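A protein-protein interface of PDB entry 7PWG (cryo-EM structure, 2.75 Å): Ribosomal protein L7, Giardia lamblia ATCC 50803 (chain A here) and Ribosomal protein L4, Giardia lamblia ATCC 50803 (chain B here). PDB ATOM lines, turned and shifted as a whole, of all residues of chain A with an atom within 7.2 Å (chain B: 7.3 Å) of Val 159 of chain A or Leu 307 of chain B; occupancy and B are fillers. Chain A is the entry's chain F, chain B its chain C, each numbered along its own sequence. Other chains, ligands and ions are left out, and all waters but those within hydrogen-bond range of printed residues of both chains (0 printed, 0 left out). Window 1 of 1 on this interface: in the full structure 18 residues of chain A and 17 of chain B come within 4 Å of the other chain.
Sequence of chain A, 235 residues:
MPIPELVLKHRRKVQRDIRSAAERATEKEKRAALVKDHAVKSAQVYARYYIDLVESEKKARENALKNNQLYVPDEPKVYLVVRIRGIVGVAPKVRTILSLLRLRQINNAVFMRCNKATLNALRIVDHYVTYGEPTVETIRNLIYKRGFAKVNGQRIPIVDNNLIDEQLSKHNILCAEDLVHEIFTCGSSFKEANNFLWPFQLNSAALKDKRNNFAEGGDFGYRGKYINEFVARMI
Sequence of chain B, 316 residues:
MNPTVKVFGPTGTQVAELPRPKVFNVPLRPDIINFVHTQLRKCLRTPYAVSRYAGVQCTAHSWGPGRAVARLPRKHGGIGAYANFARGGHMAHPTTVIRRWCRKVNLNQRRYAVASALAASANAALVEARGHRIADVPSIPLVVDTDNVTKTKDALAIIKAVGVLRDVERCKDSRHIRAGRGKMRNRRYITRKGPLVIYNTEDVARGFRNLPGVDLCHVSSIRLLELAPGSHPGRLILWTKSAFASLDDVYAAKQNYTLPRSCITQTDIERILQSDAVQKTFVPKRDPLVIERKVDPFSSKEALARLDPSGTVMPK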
ATOM      1  N   ALA A  39      -3.682  -1.463   7.065  1.00  0.00           N
ATOM      2  CA  ALA A  39      -3.098  -2.737   6.675  1.00  0.00           C
ATOM      3  C   ALA A  39      -4.159  -3.789   6.383  1.00  0.00           C
ATOM      4  O   ALA A  39      -3.942  -4.662   5.539  1.00  0.00           O
ATOM      5  CB  ALA A  39      -2.153  -3.223   7.769  1.00  0.00           C
ATOM      6  N   ARG A 140       7.171 -11.804  -1.889  1.00  0.00           N
ATOM      7  CA  ARG A 140       6.693 -11.789  -0.510  1.00  0.00           C
ATOM      8  C   ARG A 140       7.649 -12.520   0.433  1.00  0.00           C
ATOM      9  O   ARG A 140       7.997 -12.001   1.495  1.00  0.00           O
ATOM     10  CB  ARG A 140       5.288 -12.393  -0.434  1.00  0.00           C
ATOM     11  CG  ARG A 140       4.709 -12.447   0.989  1.00  0.00           C
ATOM     12  CD  ARG A 140       3.246 -12.933   1.053  1.00  0.00           C
ATOM     13  NE  ARG A 140       2.304 -11.945   0.538  1.00  0.00           N
ATOM     14  CZ  ARG A 140       1.577 -12.097  -0.564  1.00  0.00           C
ATOM     15  NH1 ARG A 140       0.764 -11.132  -0.955  1.00  0.00           N
ATOM     16  NH2 ARG A 140       1.659 -13.212  -1.270  1.00  0.00           N
ATOM     17  N   ILE A 143      10.985 -10.486   1.176  1.00  0.00           N
ATOM     18  CA  ILE A 143      10.848  -9.367   2.100  1.00  0.00           C
ATOM     19  C   ILE A 143      10.520  -9.855   3.505  1.00  0.00           C
ATOM     20  O   ILE A 143      11.113  -9.395   4.487  1.00  0.00           O
ATOM     21  CB  ILE A 143       9.801  -8.372   1.577  1.00  0.00           C
ATOM     22  CG1 ILE A 143      10.327  -7.688   0.312  1.00  0.00           C
ATOM     23  CG2 ILE A 143       9.500  -7.340   2.621  1.00  0.00           C
ATOM     24  CD1 ILE A 143       9.361  -6.744  -0.335  1.00  0.00           C
ATOM     25  N   TYR A 144       9.582 -10.794   3.635  1.00  0.00           N
ATOM     26  CA  TYR A 144       9.188 -11.220   4.971  1.00  0.00           C
ATOM     27  C   TYR A 144      10.292 -12.003   5.668  1.00  0.00           C
ATOM     28  O   TYR A 144      10.364 -11.992   6.897  1.00  0.00           O
ATOM     29  CB  TYR A 144       7.912 -12.055   4.919  1.00  0.00           C
ATOM     30  CG  TYR A 144       6.630 -11.278   4.725  1.00  0.00           C
ATOM     31  CD1 TYR A 144       6.478 -10.414   3.662  1.00  0.00           C
ATOM     32  CD2 TYR A 144       5.567 -11.430   5.592  1.00  0.00           C
ATOM     33  CE1 TYR A 144       5.326  -9.722   3.473  1.00  0.00           C
ATOM     34  CE2 TYR A 144       4.399 -10.739   5.399  1.00  0.00           C
ATOM     35  CZ  TYR A 144       4.287  -9.883   4.333  1.00  0.00           C
ATOM     36  OH  TYR A 144       3.134  -9.183   4.118  1.00  0.00           O
ATOM     37  N   LYS A 145      11.164 -12.675   4.922  1.00  0.00           N
ATOM     38  CA  LYS A 145      12.179 -13.526   5.530  1.00  0.00           C
ATOM     39  C   LYS A 145      13.593 -12.978   5.449  1.00  0.00           C
ATOM     40  O   LYS A 145      14.381 -13.211   6.365  1.00  0.00           O
ATOM     41  CB  LYS A 145      12.162 -14.917   4.892  1.00  0.00           C
ATOM     42  CG  LYS A 145      10.918 -15.706   5.187  1.00  0.00           C
ATOM     43  CD  LYS A 145      11.105 -17.157   4.819  1.00  0.00           C
ATOM     44  CE  LYS A 145       9.833 -17.758   4.270  1.00  0.00           C
ATOM     45  NZ  LYS A 145      10.047 -19.143   3.786  1.00  0.00           N
ATOM     46  N   GLY A 147      14.210  -9.592   4.643  1.00  0.00           N
ATOM     47  CA  GLY A 147      14.055  -8.152   4.567  1.00  0.00           C
ATOM     48  C   GLY A 147      14.702  -7.335   5.664  1.00  0.00           C
ATOM     49  O   GLY A 147      14.354  -7.454   6.839  1.00  0.00           O
ATOM     50  N   ILE A 156      18.895  -2.504   9.181  1.00  0.00           N
ATOM     51  CA  ILE A 156      17.940  -2.599  10.284  1.00  0.00           C
ATOM     52  C   ILE A 156      16.942  -3.712   9.978  1.00  0.00           C
ATOM     53  O   ILE A 156      16.304  -3.683   8.921  1.00  0.00           O
ATOM     54  CB  ILE A 156      17.215  -1.265  10.502  1.00  0.00           C
ATOM     55  CG1 ILE A 156      18.229  -0.130  10.598  1.00  0.00           C
ATOM     56  CG2 ILE A 156      16.389  -1.322  11.739  1.00  0.00           C
ATOM     57  CD1 ILE A 156      19.160  -0.246  11.788  1.00  0.00           C
ATOM     58  N   PRO A 157      16.767  -4.693  10.861  1.00  0.00           N
ATOM     59  CA  PRO A 157      15.775  -5.748  10.606  1.00  0.00           C
ATOM     60  C   PRO A 157      14.383  -5.178  10.383  1.00  0.00           C
ATOM     61  O   PRO A 157      13.931  -4.300  11.114  1.00  0.00           O
ATOM     62  CB  PRO A 157      15.841  -6.598  11.876  1.00  0.00           C
ATOM     63  CG  PRO A 157      17.197  -6.388  12.389  1.00  0.00           C
ATOM     64  CD  PRO A 157      17.604  -5.000  12.026  1.00  0.00           C
ATOM     65  N   ILE A 158      13.711  -5.680   9.350  1.00  0.00           N
ATOM     66  CA  ILE A 158      12.334  -5.300   9.029  1.00  0.00           C
ATOM     67  C   ILE A 158      11.422  -6.341   9.660  1.00  0.00           C
ATOM     68  O   ILE A 158      11.365  -7.484   9.205  1.00  0.00           O
ATOM     69  CB  ILE A 158      12.086  -5.212   7.516  1.00  0.00           C
ATOM     70  CG1 ILE A 158      12.994  -4.189   6.850  1.00  0.00           C
ATOM     71  CG2 ILE A 158      10.646  -4.838   7.247  1.00  0.00           C
ATOM     72  CD1 ILE A 158      12.723  -4.026   5.363  1.00  0.00           C
ATOM     73  N   VAL A 159      10.703  -5.961  10.710  1.00  0.00           N
ATOM     74  CA  VAL A 159       9.936  -6.943  11.465  1.00  0.00           C
ATOM     75  C   VAL A 159       8.487  -6.509  11.646  1.00  0.00           C
ATOM     76  O   VAL A 159       7.636  -7.327  12.002  1.00  0.00           O
ATOM     77  CB  VAL A 159      10.604  -7.222  12.824  1.00  0.00           C
ATOM     78  CG1 VAL A 159      11.848  -8.060  12.640  1.00  0.00           C
ATOM     79  CG2 VAL A 159      10.951  -5.933  13.515  1.00  0.00           C
ATOM     80  N   ASP A 160       8.183  -5.237  11.400  1.00  0.00           N
ATOM     81  CA  ASP A 160       6.824  -4.756  11.608  1.00  0.00           C
ATOM     82  C   ASP A 160       6.560  -3.535  10.739  1.00  0.00           C
ATOM     83  O   ASP A 160       7.473  -2.932  10.180  1.00  0.00           O
ATOM     84  CB  ASP A 160       6.567  -4.438  13.076  1.00  0.00           C
ATOM     85  CG  ASP A 160       7.275  -3.198  13.531  1.00  0.00           C
ATOM     86  OD1 ASP A 160       8.339  -2.872  12.969  1.00  0.00           O
ATOM     87  OD2 ASP A 160       6.778  -2.546  14.460  1.00  0.00           O
ATOM     88  N   ASN A 161       5.279  -3.172  10.653  1.00  0.00           N
ATOM     89  CA  ASN A 161       4.806  -2.057   9.846  1.00  0.00           C
ATOM     90  C   ASN A 161       5.203  -0.697  10.396  1.00  0.00           C
ATOM     91  O   ASN A 161       4.977   0.308   9.715  1.00  0.00           O
ATOM     92  CB  ASN A 161       3.287  -2.097   9.727  1.00  0.00           C
ATOM     93  CG  ASN A 161       2.798  -3.217   8.855  1.00  0.00           C
ATOM     94  OD1 ASN A 161       3.388  -3.522   7.822  1.00  0.00           O
ATOM     95  ND2 ASN A 161       1.700  -3.836   9.260  1.00  0.00           N
ATOM     96  N   ASN A 162       5.750  -0.629  11.609  1.00  0.00           N
ATOM     97  CA  ASN A 162       6.098   0.664  12.187  1.00  0.00           C
ATOM     98  C   ASN A 162       7.260   1.322  11.454  1.00  0.00           C
ATOM     99  O   ASN A 162       7.375   2.550  11.459  1.00  0.00           O
ATOM    100  CB  ASN A 162       6.442   0.508  13.662  1.00  0.00           C
ATOM    101  CG  ASN A 162       5.281  -0.010  14.487  1.00  0.00           C
ATOM    102  OD1 ASN A 162       4.123   0.361  14.277  1.00  0.00           O
ATOM    103  ND2 ASN A 162       5.590  -0.874  15.439  1.00  0.00           N
ATOM    104  N   LEU A 163       8.133   0.534  10.833  1.00  0.00           N
ATOM    105  CA  LEU A 163       9.332   1.075  10.206  1.00  0.00           C
ATOM    106  C   LEU A 163       9.137   1.377   8.731  1.00  0.00           C
ATOM    107  O   LEU A 163       9.828   2.239   8.193  1.00  0.00           O
ATOM    108  CB  LEU A 163      10.498   0.105  10.387  1.00  0.00           C
ATOM    109  CG  LEU A 163      11.916   0.627  10.161  1.00  0.00           C
ATOM    110  CD1 LEU A 163      12.258   1.650  11.204  1.00  0.00           C
ATOM    111  CD2 LEU A 163      12.893  -0.508  10.203  1.00  0.00           C
ATOM    112  N   ILE A 164       8.214   0.689   8.061  1.00  0.00           N
ATOM    113  CA  ILE A 164       7.916   1.041   6.681  1.00  0.00           C
ATOM    114  C   ILE A 164       7.111   2.331   6.617  1.00  0.00           C
ATOM    115  O   ILE A 164       7.216   3.088   5.650  1.00  0.00           O
ATOM    116  CB  ILE A 164       7.191  -0.115   5.978  1.00  0.00           C
ATOM    117  CG1 ILE A 164       7.796  -1.445   6.401  1.00  0.00           C
ATOM    118  CG2 ILE A 164       7.295   0.027   4.480  1.00  0.00           C
ATOM    119  CD1 ILE A 164       7.288  -2.596   5.607  1.00  0.00           C
ATOM    120  N   CYS A 175       2.495  -0.110   4.848  1.00  0.00           N
ATOM    121  CA  CYS A 175       2.612  -1.434   5.438  1.00  0.00           C
ATOM    122  C   CYS A 175       3.455  -2.319   4.530  1.00  0.00           C
ATOM    123  O   CYS A 175       3.888  -1.912   3.450  1.00  0.00           O
ATOM    124  CB  CYS A 175       1.233  -2.059   5.706  1.00  0.00           C
ATOM    125  SG  CYS A 175       0.246  -2.467   4.255  1.00  0.00           S
ATOM    126  N   ALA A 176       3.692  -3.548   4.987  1.00  0.00           N
ATOM    127  CA  ALA A 176       4.518  -4.476   4.229  1.00  0.00           C
ATOM    128  C   ALA A 176       3.864  -4.877   2.915  1.00  0.00           C
ATOM    129  O   ALA A 176       4.568  -5.130   1.934  1.00  0.00           O
ATOM    130  CB  ALA A 176       4.828  -5.709   5.072  1.00  0.00           C
ATOM    131  N   GLU A 177       2.535  -4.931   2.865  1.00  0.00           N
ATOM    132  CA  GLU A 177       1.851  -5.310   1.639  1.00  0.00           C
ATOM    133  C   GLU A 177       1.709  -4.167   0.644  1.00  0.00           C
ATOM    134  O   GLU A 177       1.331  -4.418  -0.499  1.00  0.00           O
ATOM    135  CB  GLU A 177       0.479  -5.891   1.963  1.00  0.00           C
ATOM    136  CG  GLU A 177       0.534  -7.300   2.539  1.00  0.00           C
ATOM    137  CD  GLU A 177       0.950  -8.340   1.512  1.00  0.00           C
ATOM    138  OE1 GLU A 177       0.922  -8.037   0.303  1.00  0.00           O
ATOM    139  OE2 GLU A 177       1.305  -9.464   1.907  1.00  0.00           O
ATOM    140  N   VAL B 290      14.015   2.190  16.916  1.00  0.00           N
ATOM    141  CA  VAL B 290      13.845   1.009  17.753  1.00  0.00           C
ATOM    142  C   VAL B 290      14.252  -0.208  16.938  1.00  0.00           C
ATOM    143  O   VAL B 290      13.763  -0.410  15.818  1.00  0.00           O
ATOM    144  CB  VAL B 290      12.404   0.882  18.276  1.00  0.00           C
ATOM    145  CG1 VAL B 290      12.224  -0.418  19.026  1.00  0.00           C
ATOM    146  CG2 VAL B 290      12.094   2.042  19.192  1.00  0.00           C
ATOM    147  N   ILE B 291      15.156  -1.006  17.491  1.00  0.00           N
ATOM    148  CA  ILE B 291      15.864  -2.034  16.746  1.00  0.00           C
ATOM    149  C   ILE B 291      15.636  -3.376  17.421  1.00  0.00           C
ATOM    150  O   ILE B 291      15.882  -3.527  18.623  1.00  0.00           O
ATOM    151  CB  ILE B 291      17.362  -1.700  16.645  1.00  0.00           C
ATOM    152  CG1 ILE B 291      17.579  -0.619  15.585  1.00  0.00           C
ATOM    153  CG2 ILE B 291      18.171  -2.929  16.358  1.00  0.00           C
ATOM    154  CD1 ILE B 291      18.699   0.314  15.890  1.00  0.00           C
ATOM    155  N   GLU B 292      15.167  -4.341  16.649  1.00  0.00           N
ATOM    156  CA  GLU B 292      14.995  -5.708  17.095  1.00  0.00           C
ATOM    157  C   GLU B 292      15.928  -6.605  16.296  1.00  0.00           C
ATOM    158  O   GLU B 292      16.663  -6.149  15.427  1.00  0.00           O
ATOM    159  CB  GLU B 292      13.538  -6.150  16.953  1.00  0.00           C
ATOM    160  CG  GLU B 292      12.560  -5.309  17.770  1.00  0.00           C
ATOM    161  CD  GLU B 292      11.284  -6.052  18.130  1.00  0.00           C
ATOM    162  OE1 GLU B 292      11.304  -7.296  18.215  1.00  0.00           O
ATOM    163  OE2 GLU B 292      10.255  -5.382  18.339  1.00  0.00           O
ATOM    164  N   ARG B 293      15.916  -7.886  16.618  1.00  0.00           N
ATOM    165  CA  ARG B 293      16.616  -8.843  15.787  1.00  0.00           C
ATOM    166  C   ARG B 293      15.669  -9.411  14.740  1.00  0.00           C
ATOM    167  O   ARG B 293      14.448  -9.408  14.902  1.00  0.00           O
ATOM    168  CB  ARG B 293      17.214  -9.962  16.630  1.00  0.00           C
ATOM    169  CG  ARG B 293      18.335  -9.498  17.532  1.00  0.00           C
ATOM    170  CD  ARG B 293      19.527  -8.977  16.735  1.00  0.00           C
ATOM    171  NE  ARG B 293      20.337 -10.078  16.237  1.00  0.00           N
ATOM    172  CZ  ARG B 293      21.182 -10.782  16.982  1.00  0.00           C
ATOM    173  NH1 ARG B 293      21.341 -10.500  18.272  1.00  0.00           N
ATOM    174  NH2 ARG B 293      21.866 -11.773  16.441  1.00  0.00           N
ATOM    175  N   LYS B 294      16.250  -9.890  13.648  1.00  0.00           N
ATOM    176  CA  LYS B 294      15.470 -10.608  12.656  1.00  0.00           C
ATOM    177  C   LYS B 294      14.967 -11.926  13.241  1.00  0.00           C
ATOM    178  O   LYS B 294      15.580 -12.511  14.139  1.00  0.00           O
ATOM    179  CB  LYS B 294      16.308 -10.858  11.403  1.00  0.00           C
ATOM    180  CG  LYS B 294      15.502 -11.172  10.150  1.00  0.00           C
ATOM    181  CD  LYS B 294      14.446 -10.128   9.877  1.00  0.00           C
ATOM    182  CE  LYS B 294      13.592 -10.521   8.707  1.00  0.00           C
ATOM    183  NZ  LYS B 294      12.553  -9.523   8.412  1.00  0.00           N
ATOM    184  N   VAL B 295      13.810 -12.359  12.760  1.00  0.00           N
ATOM    185  CA  VAL B 295      13.277 -13.682  13.060  1.00  0.00           C
ATOM    186  C   VAL B 295      12.163 -13.952  12.065  1.00  0.00           C
ATOM    187  O   VAL B 295      11.554 -13.015  11.547  1.00  0.00           O
ATOM    188  CB  VAL B 295      12.776 -13.805  14.512  1.00  0.00           C
ATOM    189  CG1 VAL B 295      11.455 -13.093  14.693  1.00  0.00           C
ATOM    190  CG2 VAL B 295      12.664 -15.260  14.887  1.00  0.00           C
ATOM    191  N   ASP B 296      11.901 -15.221  11.784  1.00  0.00           N
ATOM    192  CA  ASP B 296      10.974 -15.610  10.730  1.00  0.00           C
ATOM    193  C   ASP B 296       9.540 -15.338  11.159  1.00  0.00           C
ATOM    194  O   ASP B 296       9.073 -15.960  12.121  1.00  0.00           O
ATOM    195  CB  ASP B 296      11.174 -17.093  10.402  1.00  0.00           C
ATOM    196  CG  ASP B 296      10.415 -17.542   9.156  1.00  0.00           C
ATOM    197  OD1 ASP B 296       9.609 -16.759   8.609  1.00  0.00           O
ATOM    198  OD2 ASP B 296      10.633 -18.687   8.714  1.00  0.00           O
ATOM    199  N   PRO B 297       8.809 -14.433  10.500  1.00  0.00           N
ATOM    200  CA  PRO B 297       7.393 -14.248  10.849  1.00  0.00           C
ATOM    201  C   PRO B 297       6.549 -15.492  10.663  1.00  0.00           C
ATOM    202  O   PRO B 297       5.651 -15.739  11.476  1.00  0.00           O
ATOM    203  CB  PRO B 297       6.941 -13.114   9.917  1.00  0.00           C
ATOM    204  CG  PRO B 297       7.977 -12.966   8.920  1.00  0.00           C
ATOM    205  CD  PRO B 297       9.252 -13.467   9.487  1.00  0.00           C
ATOM    206  N   GLU B 302       1.497 -15.149  15.816  1.00  0.00           N
ATOM    207  CA  GLU B 302       1.697 -13.829  16.407  1.00  0.00           C
ATOM    208  C   GLU B 302       2.814 -13.063  15.713  1.00  0.00           C
ATOM    209  O   GLU B 302       2.699 -11.854  15.487  1.00  0.00           O
ATOM    210  CB  GLU B 302       1.995 -13.967  17.897  1.00  0.00           C
ATOM    211  CG  GLU B 302       0.914 -14.676  18.671  1.00  0.00           C
ATOM    212  CD  GLU B 302       1.300 -16.075  19.078  1.00  0.00           C
ATOM    213  OE1 GLU B 302       2.486 -16.439  18.914  1.00  0.00           O
ATOM    214  OE2 GLU B 302       0.419 -16.814  19.564  1.00  0.00           O
ATOM    215  N   ALA B 303       3.916 -13.744  15.392  1.00  0.00           N
ATOM    216  CA  ALA B 303       5.009 -13.078  14.702  1.00  0.00           C
ATOM    217  C   ALA B 303       4.570 -12.580  13.330  1.00  0.00           C
ATOM    218  O   ALA B 303       4.909 -11.462  12.934  1.00  0.00           O
ATOM    219  CB  ALA B 303       6.208 -14.019  14.581  1.00  0.00           C
ATOM    220  N   LEU B 304       3.798 -13.388  12.601  1.00  0.00           N
ATOM    221  CA  LEU B 304       3.354 -12.988  11.269  1.00  0.00           C
ATOM    222  C   LEU B 304       2.327 -11.866  11.329  1.00  0.00           C
ATOM    223  O   LEU B 304       2.306 -10.989  10.460  1.00  0.00           O
ATOM    224  CB  LEU B 304       2.776 -14.188  10.520  1.00  0.00           C
ATOM    225  CG  LEU B 304       2.486 -13.903   9.037  1.00  0.00           C
ATOM    226  CD1 LEU B 304       3.759 -13.541   8.291  1.00  0.00           C
ATOM    227  CD2 LEU B 304       1.789 -15.062   8.375  1.00  0.00           C
ATOM    228  N   ALA B 305       1.463 -11.883  12.342  1.00  0.00           N
ATOM    229  CA  ALA B 305       0.406 -10.888  12.454  1.00  0.00           C
ATOM    230  C   ALA B 305       0.956  -9.485  12.620  1.00  0.00           C
ATOM    231  O   ALA B 305       0.247  -8.512  12.346  1.00  0.00           O
ATOM    232  CB  ALA B 305      -0.507 -11.230  13.631  1.00  0.00           C
ATOM    233  N   ARG B 306       2.204  -9.367  13.062  1.00  0.00           N
ATOM    234  CA  ARG B 306       2.818  -8.063  13.254  1.00  0.00           C
ATOM    235  C   ARG B 306       2.945  -7.307  11.932  1.00  0.00           C
ATOM    236  O   ARG B 306       2.709  -6.095  11.882  1.00  0.00           O
ATOM    237  CB  ARG B 306       4.167  -8.258  13.929  1.00  0.00           C
ATOM    238  CG  ARG B 306       4.737  -7.064  14.573  1.00  0.00           C
ATOM    239  CD  ARG B 306       6.072  -7.432  15.144  1.00  0.00           C
ATOM    240  NE  ARG B 306       6.623  -6.397  15.998  1.00  0.00           N
ATOM    241  CZ  ARG B 306       7.601  -6.615  16.862  1.00  0.00           C
ATOM    242  NH1 ARG B 306       8.056  -5.624  17.608  1.00  0.00           N
ATOM    243  NH2 ARG B 306       8.104  -7.832  16.993  1.00  0.00           N
ATOM    244  N   LEU B 307       3.288  -8.008  10.847  1.00  0.00           N
ATOM    245  CA  LEU B 307       3.320  -7.378   9.528  1.00  0.00           C
ATOM    246  C   LEU B 307       1.926  -7.243   8.924  1.00  0.00           C
ATOM    247  O   LEU B 307       1.442  -6.128   8.710  1.00  0.00           O
ATOM    248  CB  LEU B 307       4.232  -8.158   8.580  1.00  0.00           C
ATOM    249  CG  LEU B 307       5.712  -7.773   8.592  1.00  0.00           C
ATOM    250  CD1 LEU B 307       6.413  -8.382   7.424  1.00  0.00           C
ATOM    251  CD2 LEU B 307       5.847  -6.286   8.553  1.00  0.00           C
ATOM    252  N   ASP B 308       1.254  -8.362   8.651  1.00  0.00           N
ATOM    253  CA  ASP B 308      -0.108  -8.294   8.135  1.00  0.00           C
ATOM    254  C   ASP B 308      -1.110  -8.794   9.165  1.00  0.00           C
ATOM    255  O   ASP B 308      -1.085  -9.979   9.526  1.00  0.00           O
ATOM    256  CB  ASP B 308      -0.265  -9.081   6.848  1.00  0.00           C
ATOM    257  CG  ASP B 308      -1.581  -8.779   6.161  1.00  0.00           C
ATOM    258  OD1 ASP B 308      -1.765  -7.614   5.743  1.00  0.00           O
ATOM    259  OD2 ASP B 308      -2.432  -9.687   6.058  1.00  0.00           O
ATOM    260  N   PRO B 309      -2.013  -7.936   9.635  1.00  0.00           N
ATOM    261  CA  PRO B 309      -2.999  -8.353  10.647  1.00  0.00           C
ATOM    262  C   PRO B 309      -4.178  -9.115  10.063  1.00  0.00           C
ATOM    263  O   PRO B 309      -4.741 -10.001  10.712  1.00  0.00           O
ATOM    264  CB  PRO B 309      -3.457  -7.019  11.256  1.00  0.00           C
ATOM    265  CG  PRO B 309      -2.462  -5.984  10.760  1.00  0.00           C
ATOM    266  CD  PRO B 309      -2.003  -6.481   9.436  1.00  0.00           C
ATOM    267  N   SER B 310      -4.543  -8.787   8.823  1.00  0.00           N
ATOM    268  CA  SER B 310      -5.730  -9.365   8.207  1.00  0.00           C
ATOM    269  C   SER B 310      -5.649 -10.886   8.138  1.00  0.00           C
ATOM    270  O   SER B 310      -6.621 -11.579   8.452  1.00  0.00           O
ATOM    271  CB  SER B 310      -5.925  -8.772   6.814  1.00  0.00           C
ATOM    272  OG  SER B 310      -7.010  -9.384   6.150  1.00  0.00           O
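O of Ala 39 of chain A touches OD1 of Asp 308 of chain B, at 3.7 Å.
NZ of Lys 294 of chain B touches O of Tyr 144 of chain A, at 3.6 Å.
Leu 307 of chain B touches Tyr 144 of chain A.
Lys 145 of chain A touches Lys 294 of chain B (O to CE, 3.7 Å).
Lys 145 of chain A touches Asp 296 of chain B (CG to OD1, 3.8 Å).
Glu 292 of chain B touches Pro 157 of chain A.
N of Lys 294 of chain B touches CB of Pro 157 of chain A (3.8 Å).
Val 159 of chain A touches Arg 293 of chain B (CG1 to O, 3.7 Å).
O of Val 159 of chain A touches CD of Arg 306 of chain B, 3.5 Å away.
Asn 161 of chain A touches Arg 306 of chain B (ND2 to O, 3.6 Å).
Hydrophobic or aromatic side chains of chain A within 4 Å of the printed part of chain B: Ala 39, Tyr 144, Pro 157, Val 159 and Ala 176.
Along chain A the printed residues that touch a printed residue of chain B span positions 39 to 177.
Of the 17 printed residues of chain B, 10 touch a printed residue of chain A.
Hydrophobic or aromatic side chains of chain B that line the printed part of chain A: Pro 297, Leu 304, Leu 307 and Pro 309.
Among the printed residues, 21 pairs touch across the chains.
Among the printed residues, no Asp or Glu carboxylate lies within 4 Å of a Lys or Arg side-chain nitrogen of the other chain.
The backbone carbonyl oxygen of Ile 158 of chain A sits at hydrogen-bond distance from the side-chain amino group of Lys 294 of chain B.
The backbone carbonyl oxygen (O) of Leu 307 of chain B lies close to the side-chain amide oxygen (OD1) of Asn 161 of chain A (3.4 Å).
O of Gly 147 of chain A is in hydrogen-bond range of NZ of Lys 294 of chain B, 3.2 Å away.
OD1 of Asn 161 of chain A lies within hydrogen-bond range of N of Ala 176 of chain A (2.9 Å).
SG of Cys 175 of chain A sits close to N of Glu 177 of chain A (3.6 Å).
The side-chain carboxylate of Glu 292 of chain B is in salt-bridge range of the guanidinium group of Arg 306 of chain B, at 3.5 Å.
The backbone carbonyl oxygen of Gly 147 of chain A lies within hydrogen-bond range of the backbone NH of Ile 158 of chain A, at 3.1 Å.
OH of Tyr 144 of chain A sits at hydrogen-bond distance from OE2 of Glu 177 of chain A, at 2.9 Å.
O of Pro 297 of chain B is in hydrogen-bond range of N of Leu 304 of chain B (3.2 Å).
Of chain B, only Arg 293, Arg 306 and Leu 307 come within 4 Å of Val 159 of chain A.
Printed residues of chain B within 4 Å of Gly 147 of chain A: Lys 294.
Of the printed residues of chain A, Pro 309 of chain B touches Ala 39.
Printed residues of chain A within 4 Å of Arg 306 of chain B: Val 159 (3.5 Å), Asp 160 (3.5 Å) and Asn 161 (3.6 Å).
Of the printed residues of chain A, Arg 293 of chain B touches Val 159.
Ala 303 of chain B touches none of the printed residues of chain A.
The nearest printed residue of chain B that does not touch Val 159 of chain A is Glu 292 of chain B (4.3 Å).
The nearest residue of chain A that does not touch Leu 307 of chain B is Ala 39 of chain A (4.7 Å).
The nearest printed residue of chain A that does not touch Pro 297 of chain B is Lys 145 of chain A (4.9 Å).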
